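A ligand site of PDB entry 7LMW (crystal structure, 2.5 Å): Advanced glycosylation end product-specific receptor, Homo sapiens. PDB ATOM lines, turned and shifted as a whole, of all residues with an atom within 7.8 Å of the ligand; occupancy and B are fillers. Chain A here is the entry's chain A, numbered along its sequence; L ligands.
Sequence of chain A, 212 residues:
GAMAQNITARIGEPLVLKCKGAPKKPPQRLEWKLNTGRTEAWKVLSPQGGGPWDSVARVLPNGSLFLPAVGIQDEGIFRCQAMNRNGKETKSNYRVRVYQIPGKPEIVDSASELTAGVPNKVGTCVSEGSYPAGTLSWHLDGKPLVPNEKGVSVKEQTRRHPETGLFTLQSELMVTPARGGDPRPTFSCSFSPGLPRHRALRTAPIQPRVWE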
ATOM      1  N   GLY A   1       8.363  -7.653 -13.505  1.00  0.00           N
ATOM      2  CA  GLY A   1       8.337  -7.345 -12.086  1.00  0.00           C
ATOM      3  C   GLY A   1       6.954  -7.583 -11.539  1.00  0.00           C
ATOM      4  O   GLY A   1       6.219  -8.392 -12.097  1.00  0.00           O
ATOM      5  N   ALA A   2       6.578  -6.861 -10.491  1.00  0.00           N
ATOM      6  CA  ALA A   2       5.269  -6.942  -9.864  1.00  0.00           C
ATOM      7  C   ALA A   2       4.390  -5.744 -10.259  1.00  0.00           C
ATOM      8  O   ALA A   2       4.854  -4.785 -10.873  1.00  0.00           O
ATOM      9  CB  ALA A   2       5.411  -6.997  -8.328  1.00  0.00           C
ATOM     10  N   MET A   3       3.127  -5.801  -9.828  1.00  0.00           N
ATOM     11  CA  MET A   3       2.195  -4.710 -10.086  1.00  0.00           C
ATOM     12  C   MET A   3       2.682  -3.467  -9.371  1.00  0.00           C
ATOM     13  O   MET A   3       2.887  -3.503  -8.160  1.00  0.00           O
ATOM     14  CB  MET A   3       0.791  -5.073  -9.561  1.00  0.00           C
ATOM     15  CG  MET A   3      -0.047  -5.943 -10.465  1.00  0.00           C
ATOM     16  SD  MET A   3      -0.546  -4.917 -11.860  1.00  0.00           S
ATOM     17  CE  MET A   3      -1.178  -6.199 -12.938  1.00  0.00           C
ATOM     18  N   ALA A   4       2.851  -2.358 -10.100  1.00  0.00           N
ATOM     19  CA  ALA A   4       3.380  -1.149  -9.495  1.00  0.00           C
ATOM     20  C   ALA A   4       2.608   0.038 -10.013  1.00  0.00           C
ATOM     21  O   ALA A   4       1.956  -0.035 -11.048  1.00  0.00           O
ATOM     22  CB  ALA A   4       4.877  -0.926  -9.818  1.00  0.00           C
ATOM     23  N   LEU A  30       8.856   0.462   9.298  1.00  0.00           N
ATOM     24  CA  LEU A  30       8.850   0.494   7.838  1.00  0.00           C
ATOM     25  C   LEU A  30      10.256   0.387   7.263  1.00  0.00           C
ATOM     26  O   LEU A  30      11.277   0.630   7.923  1.00  0.00           O
ATOM     27  CB  LEU A  30       8.176   1.746   7.257  1.00  0.00           C
ATOM     28  CG  LEU A  30       8.789   3.124   7.384  1.00  0.00           C
ATOM     29  CD1 LEU A  30       9.753   3.346   6.238  1.00  0.00           C
ATOM     30  CD2 LEU A  30       7.640   4.103   7.271  1.00  0.00           C
ATOM     31  N   GLU A  31      10.286   0.014   5.982  1.00  0.00           N
ATOM     32  CA  GLU A  31      11.509  -0.191   5.233  1.00  0.00           C
ATOM     33  C   GLU A  31      11.291   0.241   3.803  1.00  0.00           C
ATOM     34  O   GLU A  31      10.285  -0.147   3.184  1.00  0.00           O
ATOM     35  CB  GLU A  31      11.901  -1.665   5.235  1.00  0.00           C
ATOM     36  CG  GLU A  31      13.315  -1.929   5.643  1.00  0.00           C
ATOM     37  CD  GLU A  31      13.607  -3.421   5.688  1.00  0.00           C
ATOM     38  OE1 GLU A  31      12.869  -4.192   5.043  1.00  0.00           O
ATOM     39  OE2 GLU A  31      14.558  -3.797   6.396  1.00  0.00           O
ATOM     40  N   TRP A  32      12.228   0.993   3.269  1.00  0.00           N
ATOM     41  CA  TRP A  32      12.238   1.340   1.850  1.00  0.00           C
ATOM     42  C   TRP A  32      13.336   0.541   1.196  1.00  0.00           C
ATOM     43  O   TRP A  32      14.408   0.362   1.781  1.00  0.00           O
ATOM     44  CB  TRP A  32      12.477   2.839   1.617  1.00  0.00           C
ATOM     45  CG  TRP A  32      11.250   3.636   1.660  1.00  0.00           C
ATOM     46  CD1 TRP A  32      10.769   4.339   2.734  1.00  0.00           C
ATOM     47  CD2 TRP A  32      10.322   3.854   0.587  1.00  0.00           C
ATOM     48  NE1 TRP A  32       9.605   4.974   2.397  1.00  0.00           N
ATOM     49  CE2 TRP A  32       9.306   4.712   1.091  1.00  0.00           C
ATOM     50  CE3 TRP A  32      10.253   3.418  -0.741  1.00  0.00           C
ATOM     51  CZ2 TRP A  32       8.232   5.124   0.320  1.00  0.00           C
ATOM     52  CZ3 TRP A  32       9.192   3.845  -1.523  1.00  0.00           C
ATOM     53  CH2 TRP A  32       8.188   4.674  -0.997  1.00  0.00           C
ATOM     54  N   LYS A  33      13.023   0.027   0.009  1.00  0.00           N
ATOM     55  CA  LYS A  33      13.933  -0.746  -0.825  1.00  0.00           C
ATOM     56  C   LYS A  33      13.951  -0.134  -2.215  1.00  0.00           C
ATOM     57  O   LYS A  33      12.894   0.069  -2.831  1.00  0.00           O
ATOM     58  CB  LYS A  33      13.443  -2.187  -0.925  1.00  0.00           C
ATOM     59  CG  LYS A  33      14.271  -3.122  -0.167  1.00  0.00           C
ATOM     60  CD  LYS A  33      13.523  -4.335   0.288  1.00  0.00           C
ATOM     61  CE  LYS A  33      13.229  -5.228  -0.905  1.00  0.00           C
ATOM     62  NZ  LYS A  33      13.354  -6.676  -0.553  1.00  0.00           N
ATOM     63  N   LEU A  34      15.125   0.133  -2.746  1.00  0.00           N
ATOM     64  CA  LEU A  34      15.149   0.742  -4.071  1.00  0.00           C
ATOM     65  C   LEU A  34      16.228   0.058  -4.878  1.00  0.00           C
ATOM     66  O   LEU A  34      17.204  -0.471  -4.335  1.00  0.00           O
ATOM     67  CB  LEU A  34      15.344   2.277  -3.983  1.00  0.00           C
ATOM     68  CG  LEU A  34      16.717   2.883  -3.846  1.00  0.00           C
ATOM     69  CD1 LEU A  34      16.700   4.372  -4.202  1.00  0.00           C
ATOM     70  CD2 LEU A  34      17.179   2.710  -2.415  1.00  0.00           C
ATOM     71  N   TRP A  42      19.296  -4.351  -4.792  1.00  0.00           N
ATOM     72  CA  TRP A  42      18.471  -3.587  -3.858  1.00  0.00           C
ATOM     73  C   TRP A  42      19.309  -2.830  -2.836  1.00  0.00           C
ATOM     74  O   TRP A  42      20.317  -3.332  -2.337  1.00  0.00           O
ATOM     75  CB  TRP A  42      17.487  -4.503  -3.131  1.00  0.00           C
ATOM     76  CG  TRP A  42      16.400  -5.018  -4.032  1.00  0.00           C
ATOM     77  CD1 TRP A  42      16.332  -6.251  -4.583  1.00  0.00           C
ATOM     78  CD2 TRP A  42      15.265  -4.291  -4.551  1.00  0.00           C
ATOM     79  NE1 TRP A  42      15.233  -6.361  -5.378  1.00  0.00           N
ATOM     80  CE2 TRP A  42      14.553  -5.174  -5.370  1.00  0.00           C
ATOM     81  CE3 TRP A  42      14.792  -3.001  -4.389  1.00  0.00           C
ATOM     82  CZ2 TRP A  42      13.369  -4.800  -6.013  1.00  0.00           C
ATOM     83  CZ3 TRP A  42      13.623  -2.634  -5.050  1.00  0.00           C
ATOM     84  CH2 TRP A  42      12.923  -3.531  -5.830  1.00  0.00           C
ATOM     85  N   VAL A  44      18.544  -0.798   0.826  1.00  0.00           N
ATOM     86  CA  VAL A  44      17.556  -0.640   1.877  1.00  0.00           C
ATOM     87  C   VAL A  44      17.804   0.699   2.565  1.00  0.00           C
ATOM     88  O   VAL A  44      18.935   0.993   2.968  1.00  0.00           O
ATOM     89  CB  VAL A  44      17.602  -1.796   2.894  1.00  0.00           C
ATOM     90  CG1 VAL A  44      16.656  -1.537   4.057  1.00  0.00           C
ATOM     91  CG2 VAL A  44      17.279  -3.165   2.234  1.00  0.00           C
ATOM     92  N   ILE A  77      13.086   1.145  -9.454  1.00  0.00           N
ATOM     93  CA  ILE A  77      11.984   0.615  -8.681  1.00  0.00           C
ATOM     94  C   ILE A  77      12.175   1.018  -7.229  1.00  0.00           C
ATOM     95  O   ILE A  77      13.278   0.866  -6.688  1.00  0.00           O
ATOM     96  CB  ILE A  77      11.923  -0.922  -8.772  1.00  0.00           C
ATOM     97  CG1 ILE A  77      11.725  -1.336 -10.221  1.00  0.00           C
ATOM     98  CG2 ILE A  77      10.735  -1.443  -7.925  1.00  0.00           C
ATOM     99  CD1 ILE A  77      12.004  -2.770 -10.359  1.00  0.00           C
ATOM    100  N   PHE A  78      11.109   1.507  -6.609  1.00  0.00           N
ATOM    101  CA  PHE A  78      11.124   1.961  -5.221  1.00  0.00           C
ATOM    102  C   PHE A  78       9.997   1.263  -4.513  1.00  0.00           C
ATOM    103  O   PHE A  78       8.849   1.288  -4.993  1.00  0.00           O
ATOM    104  CB  PHE A  78      10.922   3.464  -5.120  1.00  0.00           C
ATOM    105  CG  PHE A  78      12.030   4.302  -5.751  1.00  0.00           C
ATOM    106  CD1 PHE A  78      12.220   4.304  -7.113  1.00  0.00           C
ATOM    107  CD2 PHE A  78      12.826   5.126  -4.976  1.00  0.00           C
ATOM    108  CE1 PHE A  78      13.190   5.123  -7.700  1.00  0.00           C
ATOM    109  CE2 PHE A  78      13.803   5.915  -5.533  1.00  0.00           C
ATOM    110  CZ  PHE A  78      13.994   5.917  -6.895  1.00  0.00           C
ATOM    111  N   ARG A  79      10.303   0.628  -3.401  1.00  0.00           N
ATOM    112  CA  ARG A  79       9.363  -0.206  -2.677  1.00  0.00           C
ATOM    113  C   ARG A  79       9.314   0.166  -1.212  1.00  0.00           C
ATOM    114  O   ARG A  79      10.363   0.360  -0.564  1.00  0.00           O
ATOM    115  CB  ARG A  79       9.767  -1.663  -2.796  1.00  0.00           C
ATOM    116  CG  ARG A  79       9.190  -2.294  -3.993  1.00  0.00           C
ATOM    117  CD  ARG A  79       9.760  -3.642  -4.141  1.00  0.00           C
ATOM    118  NE  ARG A  79       9.364  -4.224  -5.417  1.00  0.00           N
ATOM    119  CZ  ARG A  79       9.443  -5.521  -5.653  1.00  0.00           C
ATOM    120  NH1 ARG A  79       9.903  -6.357  -4.730  1.00  0.00           N
ATOM    121  NH2 ARG A  79       9.035  -5.993  -6.821  1.00  0.00           N
ATOM    122  N   CYS A  80       8.112   0.171  -0.647  1.00  0.00           N
ATOM    123  CA  CYS A  80       7.964   0.369   0.779  1.00  0.00           C
ATOM    124  C   CYS A  80       7.166  -0.776   1.351  1.00  0.00           C
ATOM    125  O   CYS A  80       6.338  -1.389   0.660  1.00  0.00           O
ATOM    126  CB  CYS A  80       7.278   1.691   1.142  1.00  0.00           C
ATOM    127  SG  CYS A  80       7.628   2.046   2.872  1.00  0.00           S
ATOM    128  N   GLN A  81       7.493  -1.110   2.589  1.00  0.00           N
ATOM    129  CA  GLN A  81       6.808  -2.129   3.365  1.00  0.00           C
ATOM    130  C   GLN A  81       6.598  -1.567   4.764  1.00  0.00           C
ATOM    131  O   GLN A  81       7.566  -1.095   5.378  1.00  0.00           O
ATOM    132  CB  GLN A  81       7.632  -3.412   3.410  1.00  0.00           C
ATOM    133  N   ALA A  82       5.358  -1.605   5.277  1.00  0.00           N
ATOM    134  CA  ALA A  82       5.057  -0.981   6.569  1.00  0.00           C
ATOM    135  C   ALA A  82       4.086  -1.829   7.379  1.00  0.00           C
ATOM    136  O   ALA A  82       3.303  -2.614   6.824  1.00  0.00           O
ATOM    137  CB  ALA A  82       4.500   0.427   6.390  1.00  0.00           C
ATOM    138  N   THR A  90       1.507  -3.441   4.924  1.00  0.00           N
ATOM    139  CA  THR A  90       1.135  -2.822   3.665  1.00  0.00           C
ATOM    140  C   THR A  90       2.389  -2.630   2.823  1.00  0.00           C
ATOM    141  O   THR A  90       3.459  -2.257   3.328  1.00  0.00           O
ATOM    142  CB  THR A  90       0.421  -1.493   3.903  1.00  0.00           C
ATOM    143  OG1 THR A  90      -0.458  -1.636   5.032  1.00  0.00           O
ATOM    144  CG2 THR A  90      -0.352  -1.055   2.649  1.00  0.00           C
ATOM    145  N   LYS A  91       2.251  -2.899   1.528  1.00  0.00           N
ATOM    146  CA  LYS A  91       3.344  -2.824   0.579  1.00  0.00           C
ATOM    147  C   LYS A  91       3.024  -1.737  -0.448  1.00  0.00           C
ATOM    148  O   LYS A  91       1.862  -1.485  -0.754  1.00  0.00           O
ATOM    149  CB  LYS A  91       3.521  -4.195  -0.068  1.00  0.00           C
ATOM    150  CG  LYS A  91       4.554  -5.063   0.631  1.00  0.00           C
ATOM    151  CD  LYS A  91       4.585  -6.460   0.069  1.00  0.00           C
ATOM    152  CE  LYS A  91       5.809  -7.246   0.559  1.00  0.00           C
ATOM    153  NZ  LYS A  91       5.773  -7.645   2.004  1.00  0.00           N
ATOM    154  N   SER A  92       4.050  -1.013  -0.913  1.00  0.00           N
ATOM    155  CA  SER A  92       3.893   0.023  -1.933  1.00  0.00           C
ATOM    156  C   SER A  92       4.984  -0.152  -2.963  1.00  0.00           C
ATOM    157  O   SER A  92       6.146  -0.346  -2.611  1.00  0.00           O
ATOM    158  CB  SER A  92       3.977   1.431  -1.344  1.00  0.00           C
ATOM    159  OG  SER A  92       3.273   1.490  -0.118  1.00  0.00           O
ATOM    160  N   ASN A  93       4.624  -0.095  -4.238  1.00  0.00           N
ATOM    161  CA  ASN A  93       5.535  -0.474  -5.295  1.00  0.00           C
ATOM    162  C   ASN A  93       5.445   0.540  -6.416  1.00  0.00           C
ATOM    163  O   ASN A  93       4.379   0.721  -7.009  1.00  0.00           O
ATOM    164  CB  ASN A  93       5.177  -1.882  -5.781  1.00  0.00           C
ATOM    165  CG  ASN A  93       6.252  -2.501  -6.641  1.00  0.00           C
ATOM    166  OD1 ASN A  93       7.456  -2.280  -6.443  1.00  0.00           O
ATOM    167  ND2 ASN A  93       5.818  -3.239  -7.678  1.00  0.00           N
ATOM    168  N   TYR A  94       6.596   1.167  -6.754  1.00  0.00           N
ATOM    169  CA  TYR A  94       6.647   2.246  -7.727  1.00  0.00           C
ATOM    170  C   TYR A  94       7.706   1.975  -8.800  1.00  0.00           C
ATOM    171  O   TYR A  94       8.834   1.575  -8.485  1.00  0.00           O
ATOM    172  CB  TYR A  94       6.968   3.565  -7.038  1.00  0.00           C
ATOM    173  CG  TYR A  94       6.022   3.978  -5.940  1.00  0.00           C
ATOM    174  CD1 TYR A  94       4.796   4.581  -6.228  1.00  0.00           C
ATOM    175  CD2 TYR A  94       6.345   3.765  -4.598  1.00  0.00           C
ATOM    176  CE1 TYR A  94       3.945   4.953  -5.235  1.00  0.00           C
ATOM    177  CE2 TYR A  94       5.488   4.151  -3.604  1.00  0.00           C
ATOM    178  CZ  TYR A  94       4.299   4.757  -3.917  1.00  0.00           C
ATOM    179  OH  TYR A  94       3.448   5.143  -2.906  1.00  0.00           O
HETATM  180  C1  LIG L   1       9.424  -5.048   0.469  1.00  0.00           C
HETATM  181  N1  LIG L   1      10.434  -3.425   1.563  1.00  0.00           N
HETATM  182  C2  LIG L   1       9.952  -8.050  -0.592  1.00  0.00           C
HETATM  183  C3  LIG L   1       6.000  -3.663  -2.641  1.00  0.00           C
HETATM  184  C4  LIG L   1       7.022  -3.879  -1.558  1.00  0.00           C
HETATM  185  C5  LIG L   1       7.761  -5.255  -1.513  1.00  0.00           C
HETATM  186  C6  LIG L   1       7.440  -6.230  -2.457  1.00  0.00           C
HETATM  187  C7  LIG L   1       6.367  -6.042  -3.570  1.00  0.00           C
HETATM  188  C8  LIG L   1       5.658  -4.721  -3.640  1.00  0.00           C
HETATM  189  C9  LIG L   1       8.712  -5.760  -0.680  1.00  0.00           C
HETATM  190  C10 LIG L   1       8.982  -7.042  -1.151  1.00  0.00           C
HETATM  191  C11 LIG L   1       9.793  -3.717   0.428  1.00  0.00           C
HETATM  192  C12 LIG L   1       9.893  -5.599   1.641  1.00  0.00           C
HETATM  193  C13 LIG L   1       6.094  -7.196  -4.538  1.00  0.00           C
HETATM  194  N2  LIG L   1       8.196  -7.322  -2.210  1.00  0.00           N
HETATM  195  N3  LIG L   1      10.485  -4.616   2.323  1.00  0.00           N
HETATM  196  O1  LIG L   1       9.512  -9.185  -0.312  1.00  0.00           O
HETATM  197  O2  LIG L   1      11.170  -7.733  -0.448  1.00  0.00           O
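The guanidinium group of Arg 79 sits at hydrogen-bond distance from the side-chain amide oxygen of Asn 93, at 2.9 Å.
The backbone NH of Glu 31 lies within hydrogen-bond range of the backbone carbonyl oxygen of Gln 81.
The backbone NH (N) of Arg 79 lies within hydrogen-bond range of the backbone carbonyl oxygen (O) of Lys 33 (2.7 Å).
The backbone NH of Ser 92 sits at hydrogen-bond distance from the backbone carbonyl oxygen of Cys 80 (2.8 Å).
The side-chain amide nitrogen of Asn 93 sits at hydrogen-bond distance from the backbone carbonyl oxygen of Met 3 (3.0 Å).
The side-chain sulfur (SG) of Cys 80 is in hydrogen-bond range of the indole nitrogen (NE1) of Trp 32 (3.6 Å).
CB of Ala 2 touches C13 of the ligand (3.9 Å).
Glu 31 touches the ligand (OE1 to N3, 3.6 Å).
Cys 80 touches the ligand.
Gln 81 touches the ligand (CB to N3, 3.3 Å).
Lys 91 touches the ligand.
Ser 92 touches the ligand (O to C3, 3.3 Å).
Asn 93 touches the ligand.
Along chain A the residues within 4 Å of the ligand span positions 2 to 93.
The nearest printed residue that does not touch the ligand is Trp 32 (4.9 Å).
The guanidinium group (NH1) of Arg 79 lies close to a nitrogen (N2) of the ligand, at 3.2 Å.
NZ of Lys 33 is in salt-bridge range of O2 of the ligand.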
